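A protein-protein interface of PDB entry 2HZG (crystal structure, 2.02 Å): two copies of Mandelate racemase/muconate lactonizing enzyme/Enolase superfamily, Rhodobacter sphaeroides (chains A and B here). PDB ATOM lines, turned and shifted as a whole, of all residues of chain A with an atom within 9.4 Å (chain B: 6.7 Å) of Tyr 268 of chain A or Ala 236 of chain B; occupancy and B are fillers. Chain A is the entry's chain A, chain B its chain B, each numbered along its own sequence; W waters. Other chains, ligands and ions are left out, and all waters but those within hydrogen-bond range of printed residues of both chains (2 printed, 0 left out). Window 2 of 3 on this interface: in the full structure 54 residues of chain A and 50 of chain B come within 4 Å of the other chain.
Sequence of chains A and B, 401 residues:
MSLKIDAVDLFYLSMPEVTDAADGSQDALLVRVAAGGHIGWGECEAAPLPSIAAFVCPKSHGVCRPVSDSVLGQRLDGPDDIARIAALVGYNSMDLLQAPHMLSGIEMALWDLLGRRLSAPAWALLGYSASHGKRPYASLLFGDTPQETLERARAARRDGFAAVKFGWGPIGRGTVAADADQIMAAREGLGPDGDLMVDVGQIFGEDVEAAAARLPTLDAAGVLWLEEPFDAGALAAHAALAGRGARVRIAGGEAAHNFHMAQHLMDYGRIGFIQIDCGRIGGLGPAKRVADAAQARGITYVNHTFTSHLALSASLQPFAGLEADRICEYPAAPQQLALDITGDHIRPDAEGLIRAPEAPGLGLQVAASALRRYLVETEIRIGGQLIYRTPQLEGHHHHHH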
ATOM      1  N   ALA A 232      15.013  14.507 -19.026  1.00  0.00           N
ATOM      2  CA  ALA A 232      14.058  13.402 -18.829  1.00  0.00           C
ATOM      3  C   ALA A 232      13.649  13.190 -17.364  1.00  0.00           C
ATOM      4  O   ALA A 232      12.478  12.897 -17.064  1.00  0.00           O
ATOM      5  CB  ALA A 232      14.616  12.111 -19.417  1.00  0.00           C
ATOM      6  N   GLY A 233      14.605  13.340 -16.454  1.00  0.00           N
ATOM      7  CA  GLY A 233      14.328  13.174 -15.022  1.00  0.00           C
ATOM      8  C   GLY A 233      13.742  14.381 -14.306  1.00  0.00           C
ATOM      9  O   GLY A 233      13.346  14.272 -13.141  1.00  0.00           O
ATOM     10  N   ALA A 234      13.676  15.528 -14.992  1.00  0.00           N
ATOM     11  CA  ALA A 234      13.170  16.776 -14.371  1.00  0.00           C
ATOM     12  C   ALA A 234      11.641  16.818 -14.294  1.00  0.00           C
ATOM     13  O   ALA A 234      11.000  17.603 -14.984  1.00  0.00           O
ATOM     14  CB  ALA A 234      13.710  18.008 -15.096  1.00  0.00           C
ATOM     15  N   LEU A 235      11.080  16.003 -13.408  1.00  0.00           N
ATOM     16  CA  LEU A 235       9.639  15.812 -13.311  1.00  0.00           C
ATOM     17  C   LEU A 235       8.925  17.017 -12.703  1.00  0.00           C
ATOM     18  O   LEU A 235       7.824  17.369 -13.123  1.00  0.00           O
ATOM     19  CB  LEU A 235       9.316  14.547 -12.510  1.00  0.00           C
ATOM     20  CG  LEU A 235      10.041  13.280 -12.973  1.00  0.00           C
ATOM     21  CD1 LEU A 235       9.742  12.128 -12.023  1.00  0.00           C
ATOM     22  CD2 LEU A 235       9.734  12.928 -14.445  1.00  0.00           C
ATOM     23  N   ALA A 236       9.560  17.640 -11.718  1.00  0.00           N
ATOM     24  CA  ALA A 236       9.012  18.842 -11.093  1.00  0.00           C
ATOM     25  C   ALA A 236       8.952  20.004 -12.106  1.00  0.00           C
ATOM     26  O   ALA A 236       7.975  20.752 -12.134  1.00  0.00           O
ATOM     27  CB  ALA A 236       9.817  19.220  -9.839  1.00  0.00           C
ATOM     28  N   ALA A 237       9.990  20.133 -12.935  1.00  0.00           N
ATOM     29  CA  ALA A 237       9.977  21.105 -14.040  1.00  0.00           C
ATOM     30  C   ALA A 237       8.783  20.860 -14.995  1.00  0.00           C
ATOM     31  O   ALA A 237       8.067  21.807 -15.357  1.00  0.00           O
ATOM     32  CB  ALA A 237      11.295  21.090 -14.789  1.00  0.00           C
ATOM     33  N   HIS A 238       8.574  19.605 -15.399  1.00  0.00           N
ATOM     34  CA  HIS A 238       7.423  19.213 -16.232  1.00  0.00           C
ATOM     35  C   HIS A 238       6.089  19.618 -15.597  1.00  0.00           C
ATOM     36  O   HIS A 238       5.223  20.216 -16.254  1.00  0.00           O
ATOM     37  CB  HIS A 238       7.421  17.698 -16.472  1.00  0.00           C
ATOM     38  CG  HIS A 238       8.365  17.241 -17.538  1.00  0.00           C
ATOM     39  ND1 HIS A 238       9.713  17.060 -17.315  1.00  0.00           N
ATOM     40  CD2 HIS A 238       8.147  16.887 -18.829  1.00  0.00           C
ATOM     41  CE1 HIS A 238      10.286  16.621 -18.423  1.00  0.00           C
ATOM     42  NE2 HIS A 238       9.357  16.498 -19.353  1.00  0.00           N
ATOM     43  N   ALA A 239       5.930  19.276 -14.316  1.00  0.00           N
ATOM     44  CA  ALA A 239       4.724  19.601 -13.570  1.00  0.00           C
ATOM     45  C   ALA A 239       4.528  21.120 -13.480  1.00  0.00           C
ATOM     46  O   ALA A 239       3.419  21.608 -13.653  1.00  0.00           O
ATOM     47  CB  ALA A 239       4.768  18.965 -12.139  1.00  0.00           C
ATOM     48  N   ALA A 240       5.595  21.859 -13.188  1.00  0.00           N
ATOM     49  CA  ALA A 240       5.514  23.341 -13.153  1.00  0.00           C
ATOM     50  C   ALA A 240       5.029  23.917 -14.498  1.00  0.00           C
ATOM     51  O   ALA A 240       4.136  24.760 -14.535  1.00  0.00           O
ATOM     52  CB  ALA A 240       6.863  23.949 -12.753  1.00  0.00           C
ATOM     53  N   LEU A 241       5.606  23.447 -15.599  1.00  0.00           N
ATOM     54  CA  LEU A 241       5.209  23.895 -16.930  1.00  0.00           C
ATOM     55  C   LEU A 241       3.735  23.590 -17.225  1.00  0.00           C
ATOM     56  O   LEU A 241       2.997  24.448 -17.733  1.00  0.00           O
ATOM     57  CB  LEU A 241       6.110  23.263 -18.004  1.00  0.00           C
ATOM     58  CG  LEU A 241       6.010  23.876 -19.416  1.00  0.00           C
ATOM     59  CD1 LEU A 241       6.423  25.353 -19.406  1.00  0.00           C
ATOM     60  CD2 LEU A 241       6.873  23.088 -20.406  1.00  0.00           C
ATOM     61  N   ALA A 242       3.317  22.366 -16.912  1.00  0.00           N
ATOM     62  CA  ALA A 242       1.946  21.931 -17.119  1.00  0.00           C
ATOM     63  C   ALA A 242       0.931  22.734 -16.295  1.00  0.00           C
ATOM     64  O   ALA A 242      -0.233  22.791 -16.662  1.00  0.00           O
ATOM     65  CB  ALA A 242       1.815  20.440 -16.815  1.00  0.00           C
ATOM     66  N   GLY A 243       1.368  23.340 -15.192  1.00  0.00           N
ATOM     67  CA  GLY A 243       0.466  24.104 -14.321  1.00  0.00           C
ATOM     68  C   GLY A 243       0.292  25.566 -14.704  1.00  0.00           C
ATOM     69  O   GLY A 243      -0.415  26.298 -14.029  1.00  0.00           O
ATOM     70  N   ILE A 250       1.661  18.658 -22.302  1.00  0.00           N
ATOM     71  CA  ILE A 250       3.062  18.244 -22.240  1.00  0.00           C
ATOM     72  C   ILE A 250       3.150  16.747 -22.562  1.00  0.00           C
ATOM     73  O   ILE A 250       2.289  15.961 -22.161  1.00  0.00           O
ATOM     74  CB  ILE A 250       3.739  18.590 -20.861  1.00  0.00           C
ATOM     75  CG1 ILE A 250       3.503  20.064 -20.458  1.00  0.00           C
ATOM     76  CG2 ILE A 250       5.245  18.258 -20.874  1.00  0.00           C
ATOM     77  CD1 ILE A 250       3.750  21.118 -21.549  1.00  0.00           C
ATOM     78  N   HIS A 260       9.679   2.486 -14.534  1.00  0.00           N
ATOM     79  CA  HIS A 260       9.428   3.533 -13.544  1.00  0.00           C
ATOM     80  C   HIS A 260       9.706   4.965 -14.009  1.00  0.00           C
ATOM     81  O   HIS A 260       9.032   5.878 -13.561  1.00  0.00           O
ATOM     82  CB  HIS A 260      10.054   3.203 -12.175  1.00  0.00           C
ATOM     83  CG  HIS A 260       9.260   2.182 -11.418  1.00  0.00           C
ATOM     84  ND1 HIS A 260       9.604   0.847 -11.386  1.00  0.00           N
ATOM     85  CD2 HIS A 260       8.096   2.289 -10.731  1.00  0.00           C
ATOM     86  CE1 HIS A 260       8.699   0.178 -10.691  1.00  0.00           C
ATOM     87  NE2 HIS A 260       7.776   1.031 -10.280  1.00  0.00           N
ATOM     88  N   MET A 261      10.677   5.156 -14.895  1.00  0.00           N
ATOM     89  CA  MET A 261      10.857   6.470 -15.542  1.00  0.00           C
ATOM     90  C   MET A 261       9.562   6.941 -16.238  1.00  0.00           C
ATOM     91  O   MET A 261       9.170   8.105 -16.118  1.00  0.00           O
ATOM     92  CB  MET A 261      12.002   6.433 -16.537  1.00  0.00           C
ATOM     93  CG  MET A 261      13.360   6.335 -15.875  1.00  0.00           C
ATOM     94  SD  MET A 261      14.677   6.398 -17.086  1.00  0.00           S
ATOM     95  CE  MET A 261      14.593   8.090 -17.712  1.00  0.00           C
ATOM     96  N   ALA A 262       8.885   6.028 -16.926  1.00  0.00           N
ATOM     97  CA  ALA A 262       7.609   6.347 -17.563  1.00  0.00           C
ATOM     98  C   ALA A 262       6.508   6.546 -16.507  1.00  0.00           C
ATOM     99  O   ALA A 262       5.756   7.531 -16.567  1.00  0.00           O
ATOM    100  CB  ALA A 262       7.220   5.264 -18.559  1.00  0.00           C
ATOM    101  N   GLN A 263       6.411   5.625 -15.539  1.00  0.00           N
ATOM    102  CA  GLN A 263       5.393   5.784 -14.493  1.00  0.00           C
ATOM    103  C   GLN A 263       5.539   7.080 -13.699  1.00  0.00           C
ATOM    104  O   GLN A 263       4.548   7.736 -13.390  1.00  0.00           O
ATOM    105  CB  GLN A 263       5.367   4.607 -13.524  1.00  0.00           C
ATOM    106  CG  GLN A 263       4.104   4.636 -12.675  1.00  0.00           C
ATOM    107  CD  GLN A 263       4.102   3.568 -11.601  1.00  0.00           C
ATOM    108  OE1 GLN A 263       3.244   2.691 -11.604  1.00  0.00           O
ATOM    109  NE2 GLN A 263       5.060   3.632 -10.691  1.00  0.00           N
ATOM    110  N   HIS A 264       6.777   7.427 -13.361  1.00  0.00           N
ATOM    111  CA  HIS A 264       7.043   8.670 -12.627  1.00  0.00           C
ATOM    112  C   HIS A 264       6.686   9.912 -13.422  1.00  0.00           C
ATOM    113  O   HIS A 264       6.141  10.872 -12.869  1.00  0.00           O
ATOM    114  CB  HIS A 264       8.499   8.738 -12.173  1.00  0.00           C
ATOM    115  CG  HIS A 264       8.865   7.681 -11.176  1.00  0.00           C
ATOM    116  ND1 HIS A 264      10.171   7.336 -10.902  1.00  0.00           N
ATOM    117  CD2 HIS A 264       8.094   6.893 -10.391  1.00  0.00           C
ATOM    118  CE1 HIS A 264      10.189   6.381  -9.989  1.00  0.00           C
ATOM    119  NE2 HIS A 264       8.940   6.085  -9.673  1.00  0.00           N
ATOM    120  N   LEU A 265       7.007   9.904 -14.715  1.00  0.00           N
ATOM    121  CA  LEU A 265       6.594  11.002 -15.589  1.00  0.00           C
ATOM    122  C   LEU A 265       5.080  11.157 -15.606  1.00  0.00           C
ATOM    123  O   LEU A 265       4.578  12.284 -15.502  1.00  0.00           O
ATOM    124  CB  LEU A 265       7.143  10.820 -17.023  1.00  0.00           C
ATOM    125  CG  LEU A 265       6.944  12.010 -17.968  1.00  0.00           C
ATOM    126  CD1 LEU A 265       7.689  13.274 -17.507  1.00  0.00           C
ATOM    127  CD2 LEU A 265       7.416  11.577 -19.354  1.00  0.00           C
ATOM    128  N   MET A 266       4.346  10.046 -15.713  1.00  0.00           N
ATOM    129  CA  MET A 266       2.867  10.134 -15.635  1.00  0.00           C
ATOM    130  C   MET A 266       2.375  10.617 -14.276  1.00  0.00           C
ATOM    131  O   MET A 266       1.498  11.479 -14.205  1.00  0.00           O
ATOM    132  CB  MET A 266       2.194   8.818 -15.985  1.00  0.00           C
ATOM    133  CG  MET A 266       2.459   8.388 -17.420  1.00  0.00           C
ATOM    134  SD  MET A 266       1.556   6.891 -17.860  1.00  0.00           S
ATOM    135  CE  MET A 266       2.526   5.641 -17.039  1.00  0.00           C
ATOM    136  N   ASP A 267       2.956  10.075 -13.209  1.00  0.00           N
ATOM    137  CA  ASP A 267       2.487  10.395 -11.860  1.00  0.00           C
ATOM    138  C   ASP A 267       2.933  11.747 -11.305  1.00  0.00           C
ATOM    139  O   ASP A 267       2.174  12.359 -10.578  1.00  0.00           O
ATOM    140  CB  ASP A 267       2.806   9.266 -10.879  1.00  0.00           C
ATOM    141  CG  ASP A 267       1.938   8.044 -11.120  1.00  0.00           C
ATOM    142  OD1 ASP A 267       0.869   8.180 -11.750  1.00  0.00           O
ATOM    143  OD2 ASP A 267       2.341   6.943 -10.725  1.00  0.00           O
ATOM    144  N   TYR A 268       4.146  12.197 -11.633  1.00  0.00           N
ATOM    145  CA  TYR A 268       4.657  13.462 -11.116  1.00  0.00           C
ATOM    146  C   TYR A 268       4.817  14.567 -12.185  1.00  0.00           C
ATOM    147  O   TYR A 268       4.888  15.744 -11.854  1.00  0.00           O
ATOM    148  CB  TYR A 268       5.981  13.220 -10.397  1.00  0.00           C
ATOM    149  CG  TYR A 268       5.839  12.197  -9.282  1.00  0.00           C
ATOM    150  CD1 TYR A 268       5.214  12.541  -8.084  1.00  0.00           C
ATOM    151  CD2 TYR A 268       6.306  10.890  -9.435  1.00  0.00           C
ATOM    152  CE1 TYR A 268       5.055  11.621  -7.063  1.00  0.00           C
ATOM    153  CE2 TYR A 268       6.158   9.945  -8.408  1.00  0.00           C
ATOM    154  CZ  TYR A 268       5.531  10.338  -7.219  1.00  0.00           C
ATOM    155  OH  TYR A 268       5.361   9.450  -6.177  1.00  0.00           O
ATOM    156  N   GLY A 269       4.900  14.183 -13.457  1.00  0.00           N
ATOM    157  CA  GLY A 269       5.228  15.140 -14.512  1.00  0.00           C
ATOM    158  C   GLY A 269       4.035  15.854 -15.084  1.00  0.00           C
ATOM    159  O   GLY A 269       4.197  16.828 -15.803  1.00  0.00           O
ATOM    160  N   ARG A 270       2.828  15.352 -14.801  1.00  0.00           N
ATOM    161  CA  ARG A 270       1.585  15.979 -15.293  1.00  0.00           C
ATOM    162  C   ARG A 270       1.554  16.009 -16.837  1.00  0.00           C
ATOM    163  O   ARG A 270       1.053  16.958 -17.453  1.00  0.00           O
ATOM    164  CB  ARG A 270       1.416  17.406 -14.713  1.00  0.00           C
ATOM    165  CG  ARG A 270       1.237  17.483 -13.193  1.00  0.00           C
ATOM    166  CD  ARG A 270       0.941  18.936 -12.776  1.00  0.00           C
ATOM    167  NE  ARG A 270      -0.278  19.455 -13.417  1.00  0.00           N
ATOM    168  CZ  ARG A 270      -0.819  20.644 -13.158  1.00  0.00           C
ATOM    169  NH1 ARG A 270      -0.252  21.459 -12.264  1.00  0.00           N
ATOM    170  NH2 ARG A 270      -1.926  21.023 -13.787  1.00  0.00           N
ATOM    171  N   ILE A 271       2.116  14.977 -17.459  1.00  0.00           N
ATOM    172  CA  ILE A 271       2.046  14.843 -18.914  1.00  0.00           C
ATOM    173  C   ILE A 271       0.664  14.358 -19.356  1.00  0.00           C
ATOM    174  O   ILE A 271      -0.009  13.611 -18.636  1.00  0.00           O
ATOM    175  CB  ILE A 271       3.132  13.897 -19.492  1.00  0.00           C
ATOM    176  CG1 ILE A 271       3.162  12.566 -18.712  1.00  0.00           C
ATOM    177  CG2 ILE A 271       4.491  14.594 -19.506  1.00  0.00           C
ATOM    178  CD1 ILE A 271       3.653  11.355 -19.569  1.00  0.00           C
ATOM    179  N   ARG A 297      -4.549   5.193 -15.790  1.00  0.00           N
ATOM    180  CA  ARG A 297      -4.496   6.630 -15.533  1.00  0.00           C
ATOM    181  C   ARG A 297      -5.268   7.491 -16.520  1.00  0.00           C
ATOM    182  O   ARG A 297      -5.407   8.693 -16.310  1.00  0.00           O
ATOM    183  CB  ARG A 297      -3.043   7.100 -15.537  1.00  0.00           C
ATOM    184  CG  ARG A 297      -2.285   6.760 -14.290  1.00  0.00           C
ATOM    185  CD  ARG A 297      -0.820   6.510 -14.614  1.00  0.00           C
ATOM    186  NE  ARG A 297      -0.066   6.168 -13.406  1.00  0.00           N
ATOM    187  CZ  ARG A 297       0.011   4.954 -12.875  1.00  0.00           C
ATOM    188  NH1 ARG A 297       0.696   4.789 -11.758  1.00  0.00           N
ATOM    189  NH2 ARG A 297      -0.606   3.913 -13.431  1.00  0.00           N
ATOM    190  N   ILE A 299      -4.228   8.229 -19.433  1.00  0.00           N
ATOM    191  CA  ILE A 299      -3.219   8.956 -20.202  1.00  0.00           C
ATOM    192  C   ILE A 299      -3.030   8.291 -21.570  1.00  0.00           C
ATOM    193  O   ILE A 299      -2.845   7.084 -21.660  1.00  0.00           O
ATOM    194  CB  ILE A 299      -1.873   9.069 -19.414  1.00  0.00           C
ATOM    195  CG1 ILE A 299      -2.095   9.885 -18.121  1.00  0.00           C
ATOM    196  CG2 ILE A 299      -0.754   9.703 -20.295  1.00  0.00           C
ATOM    197  CD1 ILE A 299      -0.951   9.839 -17.125  1.00  0.00           C
ATOM    198  N   VAL B 208       4.173  -1.543   2.353  1.00  0.00           N
ATOM    199  CA  VAL B 208       4.424  -0.568   3.405  1.00  0.00           C
ATOM    200  C   VAL B 208       4.175  -1.147   4.815  1.00  0.00           C
ATOM    201  O   VAL B 208       4.948  -0.892   5.733  1.00  0.00           O
ATOM    202  CB  VAL B 208       3.608   0.722   3.205  1.00  0.00           C
ATOM    203  CG1 VAL B 208       3.853   1.726   4.366  1.00  0.00           C
ATOM    204  CG2 VAL B 208       3.952   1.391   1.850  1.00  0.00           C
ATOM    205  N   PHE B 230      12.190  -0.487  -0.041  1.00  0.00           N
ATOM    206  CA  PHE B 230      11.309  -0.832  -1.163  1.00  0.00           C
ATOM    207  C   PHE B 230      12.041  -0.884  -2.494  1.00  0.00           C
ATOM    208  O   PHE B 230      13.190  -0.442  -2.590  1.00  0.00           O
ATOM    209  CB  PHE B 230      10.164   0.180  -1.258  1.00  0.00           C
ATOM    210  CG  PHE B 230       9.386   0.319   0.011  1.00  0.00           C
ATOM    211  CD1 PHE B 230       8.638  -0.760   0.512  1.00  0.00           C
ATOM    212  CD2 PHE B 230       9.412   1.523   0.726  1.00  0.00           C
ATOM    213  CE1 PHE B 230       7.918  -0.644   1.708  1.00  0.00           C
ATOM    214  CE2 PHE B 230       8.691   1.651   1.915  1.00  0.00           C
ATOM    215  CZ  PHE B 230       7.936   0.573   2.406  1.00  0.00           C
ATOM    216  N   GLY B 233      11.756   2.189  -7.553  1.00  0.00           N
ATOM    217  CA  GLY B 233      10.712   3.016  -8.176  1.00  0.00           C
ATOM    218  C   GLY B 233       9.493   3.287  -7.324  1.00  0.00           C
ATOM    219  O   GLY B 233       8.606   4.073  -7.706  1.00  0.00           O
ATOM    220  N   ALA B 234       9.439   2.627  -6.169  1.00  0.00           N
ATOM    221  CA  ALA B 234       8.286   2.719  -5.280  1.00  0.00           C
ATOM    222  C   ALA B 234       8.397   3.958  -4.380  1.00  0.00           C
ATOM    223  O   ALA B 234       8.518   3.853  -3.151  1.00  0.00           O
ATOM    224  CB  ALA B 234       8.136   1.419  -4.446  1.00  0.00           C
ATOM    225  N   LEU B 235       8.359   5.128  -5.014  1.00  0.00           N
ATOM    226  CA  LEU B 235       8.494   6.409  -4.297  1.00  0.00           C
ATOM    227  C   LEU B 235       7.379   6.675  -3.295  1.00  0.00           C
ATOM    228  O   LEU B 235       7.665   7.048  -2.159  1.00  0.00           O
ATOM    229  CB  LEU B 235       8.660   7.594  -5.274  1.00  0.00           C
ATOM    230  CG  LEU B 235       9.857   7.460  -6.232  1.00  0.00           C
ATOM    231  CD1 LEU B 235       9.914   8.589  -7.256  1.00  0.00           C
ATOM    232  CD2 LEU B 235      11.206   7.368  -5.480  1.00  0.00           C
ATOM    233  N   ALA B 236       6.122   6.490  -3.704  1.00  0.00           N
ATOM    234  CA  ALA B 236       4.995   6.682  -2.779  1.00  0.00           C
ATOM    235  C   ALA B 236       5.086   5.760  -1.542  1.00  0.00           C
ATOM    236  O   ALA B 236       4.718   6.165  -0.437  1.00  0.00           O
ATOM    237  CB  ALA B 236       3.665   6.495  -3.486  1.00  0.00           C
ATOM    238  N   ALA B 237       5.550   4.531  -1.734  1.00  0.00           N
ATOM    239  CA  ALA B 237       5.750   3.603  -0.615  1.00  0.00           C
ATOM    240  C   ALA B 237       6.795   4.162   0.370  1.00  0.00           C
ATOM    241  O   ALA B 237       6.556   4.154   1.576  1.00  0.00           O
ATOM    242  CB  ALA B 237       6.139   2.205  -1.115  1.00  0.00           C
ATOM    243  N   HIS B 238       7.920   4.671  -0.149  1.00  0.00           N
ATOM    244  CA  HIS B 238       8.950   5.326   0.684  1.00  0.00           C
ATOM    245  C   HIS B 238       8.343   6.454   1.503  1.00  0.00           C
ATOM    246  O   HIS B 238       8.532   6.514   2.725  1.00  0.00           O
ATOM    247  CB  HIS B 238      10.116   5.886  -0.150  1.00  0.00           C
ATOM    248  CG  HIS B 238      11.067   4.850  -0.642  1.00  0.00           C
ATOM    249  ND1 HIS B 238      10.820   4.083  -1.759  1.00  0.00           N
ATOM    250  CD2 HIS B 238      12.286   4.471  -0.186  1.00  0.00           C
ATOM    251  CE1 HIS B 238      11.838   3.266  -1.961  1.00  0.00           C
ATOM    252  NE2 HIS B 238      12.741   3.488  -1.025  1.00  0.00           N
ATOM    253  N   ALA B 239       7.586   7.326   0.832  1.00  0.00           N
ATOM    254  CA  ALA B 239       6.930   8.456   1.511  1.00  0.00           C
ATOM    255  C   ALA B 239       5.950   8.025   2.596  1.00  0.00           C
ATOM    256  O   ALA B 239       5.894   8.657   3.664  1.00  0.00           O
ATOM    257  CB  ALA B 239       6.225   9.378   0.486  1.00  0.00           C
ATOM    258  N   ALA B 240       5.160   6.978   2.319  1.00  0.00           N
ATOM    259  CA  ALA B 240       4.199   6.449   3.298  1.00  0.00           C
ATOM    260  C   ALA B 240       4.914   5.897   4.533  1.00  0.00           C
ATOM    261  O   ALA B 240       4.506   6.160   5.671  1.00  0.00           O
ATOM    262  CB  ALA B 240       3.332   5.352   2.658  1.00  0.00           C
ATOM    263  N   LEU B 241       5.973   5.120   4.306  1.00  0.00           N
ATOM    264  CA  LEU B 241       6.763   4.588   5.406  1.00  0.00           C
ATOM    265  C   LEU B 241       7.398   5.706   6.261  1.00  0.00           C
ATOM    266  O   LEU B 241       7.337   5.659   7.492  1.00  0.00           O
ATOM    267  CB  LEU B 241       7.842   3.636   4.885  1.00  0.00           C
ATOM    268  CG  LEU B 241       8.613   2.892   5.982  1.00  0.00           C
ATOM    269  CD1 LEU B 241       7.656   1.963   6.747  1.00  0.00           C
ATOM    270  CD2 LEU B 241       9.771   2.097   5.385  1.00  0.00           C
ATOM    271  N   HIS B 264      14.171  12.905  -6.722  1.00  0.00           N
ATOM    272  CA  HIS B 264      12.946  12.080  -6.665  1.00  0.00           C
ATOM    273  C   HIS B 264      12.809  11.432  -5.301  1.00  0.00           C
ATOM    274  O   HIS B 264      11.744  11.484  -4.701  1.00  0.00           O
ATOM    275  CB  HIS B 264      12.935  10.985  -7.741  1.00  0.00           C
ATOM    276  CG  HIS B 264      12.976  11.520  -9.137  1.00  0.00           C
ATOM    277  ND1 HIS B 264      13.397  10.768 -10.212  1.00  0.00           N
ATOM    278  CD2 HIS B 264      12.703  12.758  -9.622  1.00  0.00           C
ATOM    279  CE1 HIS B 264      13.357  11.513 -11.307  1.00  0.00           C
ATOM    280  NE2 HIS B 264      12.944  12.723 -10.972  1.00  0.00           N
ATOM    281  N   TYR B 268       9.814  13.113  -3.514  1.00  0.00           N
ATOM    282  CA  TYR B 268       8.660  12.222  -3.672  1.00  0.00           C
ATOM    283  C   TYR B 268       8.710  11.042  -2.707  1.00  0.00           C
ATOM    284  O   TYR B 268       7.671  10.533  -2.296  1.00  0.00           O
ATOM    285  CB  TYR B 268       8.534  11.724  -5.126  1.00  0.00           C
ATOM    286  CG  TYR B 268       8.516  12.845  -6.168  1.00  0.00           C
ATOM    287  CD1 TYR B 268       7.747  14.005  -5.969  1.00  0.00           C
ATOM    288  CD2 TYR B 268       9.250  12.735  -7.350  1.00  0.00           C
ATOM    289  CE1 TYR B 268       7.708  15.032  -6.926  1.00  0.00           C
ATOM    290  CE2 TYR B 268       9.224  13.755  -8.316  1.00  0.00           C
ATOM    291  CZ  TYR B 268       8.448  14.887  -8.101  1.00  0.00           C
ATOM    292  OH  TYR B 268       8.430  15.881  -9.044  1.00  0.00           O
ATOM    293  N   GLY B 269       9.919  10.608  -2.364  1.00  0.00           N
ATOM    294  CA  GLY B 269      10.104   9.518  -1.404  1.00  0.00           C
ATOM    295  C   GLY B 269      10.209   9.951   0.059  1.00  0.00           C
ATOM    296  O   GLY B 269      10.139   9.118   0.944  1.00  0.00           O
HETATM  297  O   HOH W   1       5.283  10.440  -3.582  1.00  0.00           O
HETATM  298  O   HOH W   2       5.662   6.359  -6.911  1.00  0.00           O
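Among the printed residues, merely in contact across the chains: Leu 235 of chain A with His 264 of chain B (3.4 Å), Leu 235 of chain A with Tyr 268 of chain B (3.8 Å), His 260 of chain A with Gly 233 of chain B (3.5 Å), His 264 of chain A with Leu 235 of chain B (3.5 Å), Tyr 268 of chain A with Leu 235 of chain B (3.9 Å), Tyr 268 of chain A with Ala 236 of chain B (3.9 Å) and Tyr 268 of chain A with Tyr 268 of chain B (3.6 Å).
The side-chain hydroxyl of Tyr 268 of chain B is in hydrogen-bond range of the backbone NH of Ala 236 of chain A (3.4 Å). The backbone carbonyl oxygen (O) of Gly 233 of chain A is in hydrogen-bond range of a ring nitrogen (NE2) of His 264 of chain B (2.7 Å). A ring nitrogen (NE2) of His 264 of chain A sits at hydrogen-bond distance from the backbone carbonyl oxygen (O) of Gly 233 of chain B (2.8 Å).
O of His 260 of chain A lies close to ND1 of His 264 of chain A, 3.2 Å away. N of Gly 269 of chain B lies within hydrogen-bond range of O of His 264 of chain B (3.1 Å).
Of the printed residues of chain B, Gly 233 of chain A touches His 264. Of the printed residues of chain B, Leu 235 of chain A touches His 264 (3.4 Å) and Tyr 268 (3.8 Å). Of the printed residues of chain B, His 260 of chain A touches Gly 233. Of chain B, only Leu 235, Ala 236 and Tyr 268 come within 4 Å of Tyr 268 of chain A. Ala 236 of chain B touches just one residue of chain A: Tyr 268 (3.9 Å). No residue of chain A comes within 4 Å of Ala 239 of chain B. Of the printed residues of chain A, His 264 of chain B touches Gly 233 (2.7 Å) and Leu 235 (3.4 Å). The nearest residue of chain B that does not touch Tyr 268 of chain A is Gly 269 of chain B (6.1 Å).
Leu 235 of chain A touches His 264 of chain B, and with the chains exchanged His 264 of chain A touches Leu 235 of chain B. Leu 235 of chain A touches Tyr 268 of chain B, and with the chains exchanged Tyr 268 of chain A touches Leu 235 of chain B. Ala 236 of chain A touches Tyr 268 of chain B, and with the chains exchanged Tyr 268 of chain A touches Ala 236 of chain B. Tyr 268 of chain B touches its own counterpart, Tyr 268 of chain A. Positions printed for both chains: 233, 234, 235, 236, 237, 238, 239, 240, 241, 264, 268 and 269. Of the 10 pairs that touch across the chains among the printed residues, 9 have their exchanged pair printed and touching as well.
Water W1 bridges the backbone carbonyl oxygen (O) of Tyr 268 of chain B and the side-chain hydroxyl (OH) of Tyr 268 of chain A. Water W2 lies within hydrogen-bond range of OH of Tyr 268 of chain A (3.2 Å) and N of Ala 236 of chain B (3.2 Å).
Of the 14 printed residues of chain B, 5 touch a printed residue of chain A. Hydrophobic or aromatic side chains of chain B within 4 Å of the printed part of chain A: Leu 235, His 264 and Tyr 268. Printed residues of chain A that touch a printed residue of chain B: Gly 233, Leu 235, Ala 236, His 260, His 264 and Tyr 268.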
